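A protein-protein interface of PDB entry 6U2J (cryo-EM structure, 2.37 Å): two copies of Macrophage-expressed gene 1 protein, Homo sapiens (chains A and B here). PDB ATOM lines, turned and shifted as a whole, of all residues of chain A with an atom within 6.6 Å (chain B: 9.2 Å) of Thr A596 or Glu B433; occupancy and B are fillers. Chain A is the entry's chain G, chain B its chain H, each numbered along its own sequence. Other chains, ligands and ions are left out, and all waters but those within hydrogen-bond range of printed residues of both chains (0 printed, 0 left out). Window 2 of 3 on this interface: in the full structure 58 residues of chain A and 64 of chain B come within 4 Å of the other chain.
The backbone NH (N) of Cys B432 sits at hydrogen-bond distance from the backbone carbonyl oxygen (O) of Asn A591 (2.9 Å).
The backbone NH of Val A593 is in hydrogen-bond range of the backbone carbonyl oxygen of Cys B432.
The backbone NH of Phe B436 is in hydrogen-bond range of the backbone carbonyl oxygen of Thr A596 (3.3 Å).
The backbone NH (N) of Ser A598 lies within hydrogen-bond range of the backbone carbonyl oxygen (O) of Phe B436, at 3.5 Å.
ND1 of His B419 sits at hydrogen-bond distance from O of Ile A628, at 2.8 Å.
The side-chain carboxylate (OD1) of Asp B434 lies close to the backbone carbonyl oxygen (O) of Ile A594 (3.1 Å).
The side-chain hydroxyl of Ser A603 lies close to the backbone carbonyl oxygen of Val A595.
The backbone carbonyl oxygen (O) of Val A595 is in hydrogen-bond range of the backbone NH (N) of Trp A604 (2.6 Å).
The side-chain hydroxyl of Thr A596 is in hydrogen-bond range of the backbone carbonyl oxygen of Arg A602.
The backbone carbonyl oxygen of Tyr B413 lies within hydrogen-bond range of the backbone NH of Gln B437 (3.3 Å).
The backbone carbonyl oxygen (O) of Val B435 is in hydrogen-bond range of the side-chain amide nitrogen (ND2) of Asn B414 (3.0 Å).
N of His B415 is in hydrogen-bond range of O of Val B435 (3.1 Å).
Among the printed residues, merely in contact across the chains: Thr A592 with Cys B432 (3.6 Å), Ile A594 with Glu B433 (3.6 Å), Asn A591 with Val B431 (3.6 Å), Thr A596 with Glu B433 (3.6 Å), Thr A596 with Asp B434 (3.6 Å), Asn A597 with Phe B436 (3.7 Å), Val A595 with Asp B434 (3.7 Å), Thr A596 with Val B435 (3.7 Å), Ser A598 with Gln B437 (3.8 Å), Val A595 with Phe B436 (3.9 Å), Pro A308 with Phe B436 (3.9 Å) and Asn A591 with Thr B430 (3.95 Å).
Of the printed residues of chain B, Pro A308 touches Phe B436 (3.9 Å).
Of the printed residues of chain B, Thr A592 touches Cys B432.
Of chain B, only Glu B433 (3.6 Å) and Asp B434 (3.1 Å) come within 4 Å of Ile A594.
Val A595 touches just these residues of chain B: Asp B434 (3.7 Å) and Phe B436 (3.9 Å).
Thr A596 touches four residues of chain B.
Asn A597 touches one residue of chain B.
Of the printed residues of chain B, Ser A598 touches Phe B436 and Gln B437.
Tyr B413 touches none of the printed residues of chain A.
Of the printed residues of chain A, Val B431 touches Asn A591.
Glu B433 touches just these residues of chain A: Ile A594 (3.6 Å) and Thr A596 (3.6 Å).
Of the printed residues of chain A, Val B435 touches Thr A596.
The nearest residue of chain B that does not touch Thr A596 is Gln B437 (6.2 Å).
Hydrophobic or aromatic side chains of chain B within 4 Å of the printed part of chain A: His B419 and Phe B436.
Of the 16 printed residues of chain A, 10 touch a printed residue of chain B.
Among the printed residues, 18 pairs touch across the chains.
Among the printed residues, no Asp or Glu carboxylate lies within 4 Å of a Lys or Arg side-chain nitrogen of the other chain.
No position is printed for both chains.
Of the 18 pairs that touch across the chains among the printed residues, none has its exchanged pair printed and touching as well.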
ATOM      1  N   PRO A 308      -5.991 -27.529 -17.156  1.00  0.00           N
ATOM      2  CA  PRO A 308      -6.640 -26.674 -18.163  1.00  0.00           C
ATOM      3  C   PRO A 308      -7.094 -27.415 -19.403  1.00  0.00           C
ATOM      4  O   PRO A 308      -7.808 -26.827 -20.224  1.00  0.00           O
ATOM      5  CB  PRO A 308      -5.552 -25.654 -18.509  1.00  0.00           C
ATOM      6  CG  PRO A 308      -4.626 -25.679 -17.369  1.00  0.00           C
ATOM      7  CD  PRO A 308      -4.609 -27.090 -16.904  1.00  0.00           C
ATOM      8  N   ASN A 591       1.855 -33.553 -32.053  1.00  0.00           N
ATOM      9  CA  ASN A 591       1.909 -34.269 -30.782  1.00  0.00           C
ATOM     10  C   ASN A 591       2.399 -33.341 -29.677  1.00  0.00           C
ATOM     11  O   ASN A 591       3.593 -33.041 -29.593  1.00  0.00           O
ATOM     12  CB  ASN A 591       2.815 -35.488 -30.906  1.00  0.00           C
ATOM     13  CG  ASN A 591       2.302 -36.488 -31.915  1.00  0.00           C
ATOM     14  OD1 ASN A 591       2.938 -36.737 -32.937  1.00  0.00           O
ATOM     15  ND2 ASN A 591       1.138 -37.064 -31.637  1.00  0.00           N
ATOM     16  N   THR A 592       1.481 -32.892 -28.824  1.00  0.00           N
ATOM     17  CA  THR A 592       1.856 -32.124 -27.646  1.00  0.00           C
ATOM     18  C   THR A 592       2.369 -33.066 -26.570  1.00  0.00           C
ATOM     19  O   THR A 592       1.770 -34.114 -26.313  1.00  0.00           O
ATOM     20  CB  THR A 592       0.673 -31.325 -27.109  1.00  0.00           C
ATOM     21  OG1 THR A 592      -0.363 -32.225 -26.706  1.00  0.00           O
ATOM     22  CG2 THR A 592       0.140 -30.391 -28.164  1.00  0.00           C
ATOM     23  N   VAL A 593       3.479 -32.692 -25.943  1.00  0.00           N
ATOM     24  CA  VAL A 593       4.090 -33.485 -24.892  1.00  0.00           C
ATOM     25  C   VAL A 593       3.995 -32.785 -23.542  1.00  0.00           C
ATOM     26  O   VAL A 593       3.766 -33.430 -22.516  1.00  0.00           O
ATOM     27  CB  VAL A 593       5.558 -33.808 -25.252  1.00  0.00           C
ATOM     28  CG1 VAL A 593       6.207 -34.708 -24.208  1.00  0.00           C
ATOM     29  CG2 VAL A 593       5.639 -34.440 -26.630  1.00  0.00           C
ATOM     30  N   ILE A 594       4.125 -31.463 -23.529  1.00  0.00           N
ATOM     31  CA  ILE A 594       4.117 -30.677 -22.303  1.00  0.00           C
ATOM     32  C   ILE A 594       2.890 -29.778 -22.313  1.00  0.00           C
ATOM     33  O   ILE A 594       2.695 -28.991 -23.247  1.00  0.00           O
ATOM     34  CB  ILE A 594       5.399 -29.847 -22.158  1.00  0.00           C
ATOM     35  CG1 ILE A 594       6.619 -30.758 -22.073  1.00  0.00           C
ATOM     36  CG2 ILE A 594       5.322 -28.948 -20.940  1.00  0.00           C
ATOM     37  CD1 ILE A 594       7.921 -30.013 -22.189  1.00  0.00           C
ATOM     38  N   VAL A 595       2.067 -29.894 -21.276  1.00  0.00           N
ATOM     39  CA  VAL A 595       0.952 -28.989 -21.028  1.00  0.00           C
ATOM     40  C   VAL A 595       1.274 -28.199 -19.772  1.00  0.00           C
ATOM     41  O   VAL A 595       1.608 -28.786 -18.738  1.00  0.00           O
ATOM     42  CB  VAL A 595      -0.375 -29.753 -20.868  1.00  0.00           C
ATOM     43  CG1 VAL A 595      -1.488 -28.814 -20.448  1.00  0.00           C
ATOM     44  CG2 VAL A 595      -0.746 -30.449 -22.157  1.00  0.00           C
ATOM     45  N   THR A 596       1.191 -26.874 -19.856  1.00  0.00           N
ATOM     46  CA  THR A 596       1.467 -26.043 -18.696  1.00  0.00           C
ATOM     47  C   THR A 596       0.609 -24.790 -18.753  1.00  0.00           C
ATOM     48  O   THR A 596       0.001 -24.469 -19.775  1.00  0.00           O
ATOM     49  CB  THR A 596       2.950 -25.669 -18.610  1.00  0.00           C
ATOM     50  OG1 THR A 596       3.215 -25.065 -17.340  1.00  0.00           O
ATOM     51  CG2 THR A 596       3.318 -24.687 -19.702  1.00  0.00           C
ATOM     52  N   ASN A 597       0.554 -24.087 -17.627  1.00  0.00           N
ATOM     53  CA  ASN A 597      -0.053 -22.768 -17.559  1.00  0.00           C
ATOM     54  C   ASN A 597       0.852 -21.819 -16.788  1.00  0.00           C
ATOM     55  O   ASN A 597       1.554 -22.217 -15.856  1.00  0.00           O
ATOM     56  CB  ASN A 597      -1.453 -22.806 -16.931  1.00  0.00           C
ATOM     57  CG  ASN A 597      -1.493 -23.545 -15.618  1.00  0.00           C
ATOM     58  OD1 ASN A 597      -0.496 -24.107 -15.172  1.00  0.00           O
ATOM     59  ND2 ASN A 597      -2.652 -23.527 -14.974  1.00  0.00           N
ATOM     60  N   SER A 598       0.833 -20.553 -17.195  1.00  0.00           N
ATOM     61  CA  SER A 598       1.753 -19.574 -16.637  1.00  0.00           C
ATOM     62  C   SER A 598       1.338 -19.075 -15.264  1.00  0.00           C
ATOM     63  O   SER A 598       2.195 -18.604 -14.509  1.00  0.00           O
ATOM     64  CB  SER A 598       1.884 -18.382 -17.584  1.00  0.00           C
ATOM     65  OG  SER A 598       2.731 -17.385 -17.038  1.00  0.00           O
ATOM     66  N   ALA A 601       2.338 -21.924 -12.682  1.00  0.00           N
ATOM     67  CA  ALA A 601       3.626 -22.553 -13.006  1.00  0.00           C
ATOM     68  C   ALA A 601       3.595 -24.063 -12.775  1.00  0.00           C
ATOM     69  O   ALA A 601       4.593 -24.668 -12.380  1.00  0.00           O
ATOM     70  CB  ALA A 601       4.791 -21.906 -12.247  1.00  0.00           C
ATOM     71  N   ARG A 602       2.444 -24.681 -13.023  1.00  0.00           N
ATOM     72  CA  ARG A 602       2.301 -26.126 -13.010  1.00  0.00           C
ATOM     73  C   ARG A 602       2.435 -26.643 -14.431  1.00  0.00           C
ATOM     74  O   ARG A 602       2.074 -25.962 -15.391  1.00  0.00           O
ATOM     75  CB  ARG A 602       0.950 -26.548 -12.431  1.00  0.00           C
ATOM     76  CG  ARG A 602       0.780 -26.250 -10.959  1.00  0.00           C
ATOM     77  CD  ARG A 602      -0.600 -26.656 -10.484  1.00  0.00           C
ATOM     78  NE  ARG A 602      -0.784 -28.103 -10.513  1.00  0.00           N
ATOM     79  CZ  ARG A 602      -1.952 -28.709 -10.333  1.00  0.00           C
ATOM     80  NH1 ARG A 602      -3.045 -27.993 -10.119  1.00  0.00           N
ATOM     81  NH2 ARG A 602      -2.029 -30.032 -10.372  1.00  0.00           N
ATOM     82  N   SER A 603       2.959 -27.854 -14.560  1.00  0.00           N
ATOM     83  CA  SER A 603       3.209 -28.415 -15.873  1.00  0.00           C
ATOM     84  C   SER A 603       2.948 -29.910 -15.852  1.00  0.00           C
ATOM     85  O   SER A 603       3.136 -30.577 -14.832  1.00  0.00           O
ATOM     86  CB  SER A 603       4.638 -28.140 -16.335  1.00  0.00           C
ATOM     87  OG  SER A 603       4.863 -28.708 -17.609  1.00  0.00           O
ATOM     88  N   TRP A 604       2.513 -30.428 -16.995  1.00  0.00           N
ATOM     89  CA  TRP A 604       2.189 -31.838 -17.144  1.00  0.00           C
ATOM     90  C   TRP A 604       2.970 -32.399 -18.319  1.00  0.00           C
ATOM     91  O   TRP A 604       2.947 -31.826 -19.411  1.00  0.00           O
ATOM     92  CB  TRP A 604       0.688 -32.043 -17.356  1.00  0.00           C
ATOM     93  CG  TRP A 604      -0.130 -31.716 -16.153  1.00  0.00           C
ATOM     94  CD1 TRP A 604      -0.509 -32.571 -15.166  1.00  0.00           C
ATOM     95  CD2 TRP A 604      -0.657 -30.435 -15.800  1.00  0.00           C
ATOM     96  NE1 TRP A 604      -1.249 -31.905 -14.222  1.00  0.00           N
ATOM     97  CE2 TRP A 604      -1.351 -30.590 -14.590  1.00  0.00           C
ATOM     98  CE3 TRP A 604      -0.612 -29.174 -16.394  1.00  0.00           C
ATOM     99  CZ2 TRP A 604      -1.995 -29.532 -13.962  1.00  0.00           C
ATOM    100  CZ3 TRP A 604      -1.250 -28.126 -15.770  1.00  0.00           C
ATOM    101  CH2 TRP A 604      -1.932 -28.310 -14.566  1.00  0.00           C
ATOM    102  N   LEU A 621      11.649 -30.415 -17.026  1.00  0.00           N
ATOM    103  CA  LEU A 621      11.079 -29.449 -17.962  1.00  0.00           C
ATOM    104  C   LEU A 621      12.095 -29.047 -19.020  1.00  0.00           C
ATOM    105  O   LEU A 621      11.889 -29.281 -20.216  1.00  0.00           O
ATOM    106  CB  LEU A 621      10.572 -28.216 -17.213  1.00  0.00           C
ATOM    107  CG  LEU A 621       9.298 -28.406 -16.396  1.00  0.00           C
ATOM    108  CD1 LEU A 621       8.964 -27.146 -15.617  1.00  0.00           C
ATOM    109  CD2 LEU A 621       8.176 -28.772 -17.338  1.00  0.00           C
ATOM    110  N   MET A 625      12.295 -29.319 -22.727  1.00  0.00           N
ATOM    111  CA  MET A 625      12.218 -28.096 -23.518  1.00  0.00           C
ATOM    112  C   MET A 625      13.381 -27.947 -24.488  1.00  0.00           C
ATOM    113  O   MET A 625      13.319 -27.087 -25.373  1.00  0.00           O
ATOM    114  CB  MET A 625      12.157 -26.866 -22.607  1.00  0.00           C
ATOM    115  CG  MET A 625      10.835 -26.678 -21.882  1.00  0.00           C
ATOM    116  SD  MET A 625      10.842 -25.234 -20.803  1.00  0.00           S
ATOM    117  CE  MET A 625       9.228 -25.371 -20.040  1.00  0.00           C
ATOM    118  N   ILE A 628      11.992 -29.598 -27.413  1.00  0.00           N
ATOM    119  CA  ILE A 628      10.801 -28.853 -27.797  1.00  0.00           C
ATOM    120  C   ILE A 628      11.140 -27.474 -28.344  1.00  0.00           C
ATOM    121  O   ILE A 628      10.441 -26.974 -29.232  1.00  0.00           O
ATOM    122  CB  ILE A 628       9.849 -28.720 -26.605  1.00  0.00           C
ATOM    123  N   TYR B 413      -6.909 -18.459 -23.015  1.00  0.00           N
ATOM    124  CA  TYR B 413      -6.676 -18.775 -24.414  1.00  0.00           C
ATOM    125  C   TYR B 413      -5.458 -19.684 -24.513  1.00  0.00           C
ATOM    126  O   TYR B 413      -4.830 -20.028 -23.510  1.00  0.00           O
ATOM    127  CB  TYR B 413      -6.527 -17.503 -25.257  1.00  0.00           C
ATOM    128  CG  TYR B 413      -5.379 -16.602 -24.873  1.00  0.00           C
ATOM    129  CD1 TYR B 413      -5.534 -15.623 -23.901  1.00  0.00           C
ATOM    130  CD2 TYR B 413      -4.150 -16.700 -25.511  1.00  0.00           C
ATOM    131  CE1 TYR B 413      -4.490 -14.791 -23.556  1.00  0.00           C
ATOM    132  CE2 TYR B 413      -3.105 -15.870 -25.172  1.00  0.00           C
ATOM    133  CZ  TYR B 413      -3.283 -14.912 -24.201  1.00  0.00           C
ATOM    134  OH  TYR B 413      -2.242 -14.087 -23.855  1.00  0.00           O
ATOM    135  N   ASN B 414      -5.123 -20.072 -25.738  1.00  0.00           N
ATOM    136  CA  ASN B 414      -4.164 -21.137 -25.982  1.00  0.00           C
ATOM    137  C   ASN B 414      -3.192 -20.716 -27.073  1.00  0.00           C
ATOM    138  O   ASN B 414      -3.614 -20.330 -28.168  1.00  0.00           O
ATOM    139  CB  ASN B 414      -4.893 -22.418 -26.401  1.00  0.00           C
ATOM    140  CG  ASN B 414      -4.106 -23.679 -26.105  1.00  0.00           C
ATOM    141  OD1 ASN B 414      -4.628 -24.783 -26.233  1.00  0.00           O
ATOM    142  ND2 ASN B 414      -2.863 -23.523 -25.668  1.00  0.00           N
ATOM    143  N   HIS B 415      -1.899 -20.791 -26.779  1.00  0.00           N
ATOM    144  CA  HIS B 415      -0.870 -20.752 -27.806  1.00  0.00           C
ATOM    145  C   HIS B 415      -0.474 -22.171 -28.177  1.00  0.00           C
ATOM    146  O   HIS B 415      -0.706 -23.121 -27.428  1.00  0.00           O
ATOM    147  CB  HIS B 415       0.367 -19.981 -27.346  1.00  0.00           C
ATOM    148  CG  HIS B 415       0.131 -18.522 -27.134  1.00  0.00           C
ATOM    149  ND1 HIS B 415      -0.075 -17.644 -28.175  1.00  0.00           N
ATOM    150  CD2 HIS B 415       0.104 -17.779 -26.002  1.00  0.00           C
ATOM    151  CE1 HIS B 415      -0.240 -16.425 -27.693  1.00  0.00           C
ATOM    152  NE2 HIS B 415      -0.132 -16.479 -26.377  1.00  0.00           N
ATOM    153  N   LEU B 416       0.143 -22.306 -29.346  1.00  0.00           N
ATOM    154  CA  LEU B 416       0.505 -23.626 -29.851  1.00  0.00           C
ATOM    155  C   LEU B 416       1.676 -23.429 -30.809  1.00  0.00           C
ATOM    156  O   LEU B 416       1.473 -23.011 -31.952  1.00  0.00           O
ATOM    157  CB  LEU B 416      -0.683 -24.272 -30.548  1.00  0.00           C
ATOM    158  CG  LEU B 416      -0.640 -25.761 -30.872  1.00  0.00           C
ATOM    159  CD1 LEU B 416      -0.756 -26.543 -29.594  1.00  0.00           C
ATOM    160  CD2 LEU B 416      -1.757 -26.133 -31.808  1.00  0.00           C
ATOM    161  N   GLU B 417       2.889 -23.721 -30.346  1.00  0.00           N
ATOM    162  CA  GLU B 417       4.079 -23.567 -31.170  1.00  0.00           C
ATOM    163  C   GLU B 417       4.760 -24.913 -31.379  1.00  0.00           C
ATOM    164  O   GLU B 417       4.774 -25.764 -30.484  1.00  0.00           O
ATOM    165  CB  GLU B 417       5.061 -22.549 -30.563  1.00  0.00           C
ATOM    166  CG  GLU B 417       5.711 -22.939 -29.244  1.00  0.00           C
ATOM    167  CD  GLU B 417       4.919 -22.482 -28.040  1.00  0.00           C
ATOM    168  OE1 GLU B 417       3.733 -22.129 -28.199  1.00  0.00           O
ATOM    169  OE2 GLU B 417       5.492 -22.465 -26.931  1.00  0.00           O
ATOM    170  N   CYS B 418       5.308 -25.102 -32.577  1.00  0.00           N
ATOM    171  CA  CYS B 418       5.975 -26.334 -32.964  1.00  0.00           C
ATOM    172  C   CYS B 418       7.385 -26.030 -33.444  1.00  0.00           C
ATOM    173  O   CYS B 418       7.755 -24.879 -33.686  1.00  0.00           O
ATOM    174  CB  CYS B 418       5.219 -27.069 -34.080  1.00  0.00           C
ATOM    175  SG  CYS B 418       3.622 -27.754 -33.638  1.00  0.00           S
ATOM    176  N   HIS B 419       8.166 -27.095 -33.594  1.00  0.00           N
ATOM    177  CA  HIS B 419       9.477 -27.041 -34.223  1.00  0.00           C
ATOM    178  C   HIS B 419       9.660 -28.313 -35.033  1.00  0.00           C
ATOM    179  O   HIS B 419       9.540 -29.416 -34.492  1.00  0.00           O
ATOM    180  CB  HIS B 419      10.591 -26.884 -33.182  1.00  0.00           C
ATOM    181  CG  HIS B 419      10.600 -25.547 -32.510  1.00  0.00           C
ATOM    182  ND1 HIS B 419       9.838 -25.269 -31.397  1.00  0.00           N
ATOM    183  CD2 HIS B 419      11.279 -24.410 -32.796  1.00  0.00           C
ATOM    184  CE1 HIS B 419      10.044 -24.017 -31.026  1.00  0.00           C
ATOM    185  NE2 HIS B 419      10.916 -23.475 -31.858  1.00  0.00           N
ATOM    186  N   THR B 430       7.808 -34.220 -35.285  1.00  0.00           N
ATOM    187  CA  THR B 430       7.393 -32.896 -34.836  1.00  0.00           C
ATOM    188  C   THR B 430       6.707 -32.967 -33.475  1.00  0.00           C
ATOM    189  O   THR B 430       5.584 -33.461 -33.362  1.00  0.00           O
ATOM    190  CB  THR B 430       6.438 -32.233 -35.849  1.00  0.00           C
ATOM    191  OG1 THR B 430       7.087 -32.117 -37.121  1.00  0.00           O
ATOM    192  CG2 THR B 430       6.019 -30.850 -35.373  1.00  0.00           C
ATOM    193  N   VAL B 431       7.388 -32.484 -32.443  1.00  0.00           N
ATOM    194  CA  VAL B 431       6.813 -32.390 -31.115  1.00  0.00           C
ATOM    195  C   VAL B 431       6.275 -30.980 -30.930  1.00  0.00           C
ATOM    196  O   VAL B 431       6.621 -30.050 -31.665  1.00  0.00           O
ATOM    197  CB  VAL B 431       7.829 -32.750 -30.009  1.00  0.00           C
ATOM    198  CG1 VAL B 431       8.288 -34.191 -30.161  1.00  0.00           C
ATOM    199  CG2 VAL B 431       9.010 -31.808 -30.054  1.00  0.00           C
ATOM    200  N   CYS B 432       5.409 -30.814 -29.935  1.00  0.00           N
ATOM    201  CA  CYS B 432       4.708 -29.555 -29.752  1.00  0.00           C
ATOM    202  C   CYS B 432       4.518 -29.263 -28.272  1.00  0.00           C
ATOM    203  O   CYS B 432       4.798 -30.093 -27.402  1.00  0.00           O
ATOM    204  CB  CYS B 432       3.354 -29.569 -30.460  1.00  0.00           C
ATOM    205  SG  CYS B 432       2.451 -28.034 -30.282  1.00  0.00           S
ATOM    206  N   GLU B 433       4.016 -28.062 -28.003  1.00  0.00           N
ATOM    207  CA  GLU B 433       3.809 -27.566 -26.651  1.00  0.00           C
ATOM    208  C   GLU B 433       2.746 -26.479 -26.703  1.00  0.00           C
ATOM    209  O   GLU B 433       2.743 -25.655 -27.621  1.00  0.00           O
ATOM    210  CB  GLU B 433       5.119 -27.025 -26.068  1.00  0.00           C
ATOM    211  CG  GLU B 433       5.095 -26.679 -24.588  1.00  0.00           C
ATOM    212  CD  GLU B 433       4.653 -25.258 -24.322  1.00  0.00           C
ATOM    213  OE1 GLU B 433       4.853 -24.407 -25.209  1.00  0.00           O
ATOM    214  OE2 GLU B 433       4.108 -24.990 -23.233  1.00  0.00           O
ATOM    215  N   ASP B 434       1.856 -26.479 -25.713  1.00  0.00           N
ATOM    216  CA  ASP B 434       0.784 -25.496 -25.622  1.00  0.00           C
ATOM    217  C   ASP B 434       0.753 -24.859 -24.243  1.00  0.00           C
ATOM    218  O   ASP B 434       0.734 -25.557 -23.225  1.00  0.00           O
ATOM    219  CB  ASP B 434      -0.571 -26.118 -25.954  1.00  0.00           C
ATOM    220  CG  ASP B 434      -0.784 -27.442 -25.277  1.00  0.00           C
ATOM    221  OD1 ASP B 434       0.177 -27.963 -24.686  1.00  0.00           O
ATOM    222  OD2 ASP B 434      -1.911 -27.968 -25.340  1.00  0.00           O
ATOM    223  N   VAL B 435       0.744 -23.532 -24.219  1.00  0.00           N
ATOM    224  CA  VAL B 435       0.703 -22.770 -22.982  1.00  0.00           C
ATOM    225  C   VAL B 435      -0.665 -22.107 -22.880  1.00  0.00           C
ATOM    226  O   VAL B 435      -1.284 -21.745 -23.887  1.00  0.00           O
ATOM    227  CB  VAL B 435       1.874 -21.754 -22.917  1.00  0.00           C
ATOM    228  CG1 VAL B 435       1.747 -20.658 -23.964  1.00  0.00           C
ATOM    229  CG2 VAL B 435       2.040 -21.161 -21.519  1.00  0.00           C
ATOM    230  N   PHE B 436      -1.165 -22.005 -21.654  1.00  0.00           N
ATOM    231  CA  PHE B 436      -2.470 -21.427 -21.373  1.00  0.00           C
ATOM    232  C   PHE B 436      -2.276 -20.138 -20.590  1.00  0.00           C
ATOM    233  O   PHE B 436      -1.723 -20.155 -19.487  1.00  0.00           O
ATOM    234  CB  PHE B 436      -3.337 -22.411 -20.592  1.00  0.00           C
ATOM    235  CG  PHE B 436      -3.764 -23.605 -21.388  1.00  0.00           C
ATOM    236  CD1 PHE B 436      -4.904 -23.559 -22.167  1.00  0.00           C
ATOM    237  CD2 PHE B 436      -3.010 -24.764 -21.379  1.00  0.00           C
ATOM    238  CE1 PHE B 436      -5.298 -24.654 -22.903  1.00  0.00           C
ATOM    239  CE2 PHE B 436      -3.397 -25.860 -22.117  1.00  0.00           C
ATOM    240  CZ  PHE B 436      -4.541 -25.804 -22.879  1.00  0.00           C
ATOM    241  N   GLN B 437      -2.715 -19.028 -21.165  1.00  0.00           N
ATOM    242  CA  GLN B 437      -2.624 -17.733 -20.519  1.00  0.00           C
ATOM    243  C   GLN B 437      -3.995 -17.341 -19.984  1.00  0.00           C
ATOM    244  O   GLN B 437      -4.986 -18.049 -20.168  1.00  0.00           O
ATOM    245  CB  GLN B 437      -2.111 -16.679 -21.499  1.00  0.00           C
ATOM    246  CG  GLN B 437      -0.768 -16.971 -22.133  1.00  0.00           C
ATOM    247  CD  GLN B 437       0.373 -16.910 -21.150  1.00  0.00           C
ATOM    248  OE1 GLN B 437       0.393 -16.070 -20.252  1.00  0.00           O
ATOM    249  NE2 GLN B 437       1.343 -17.795 -21.325  1.00  0.00           N
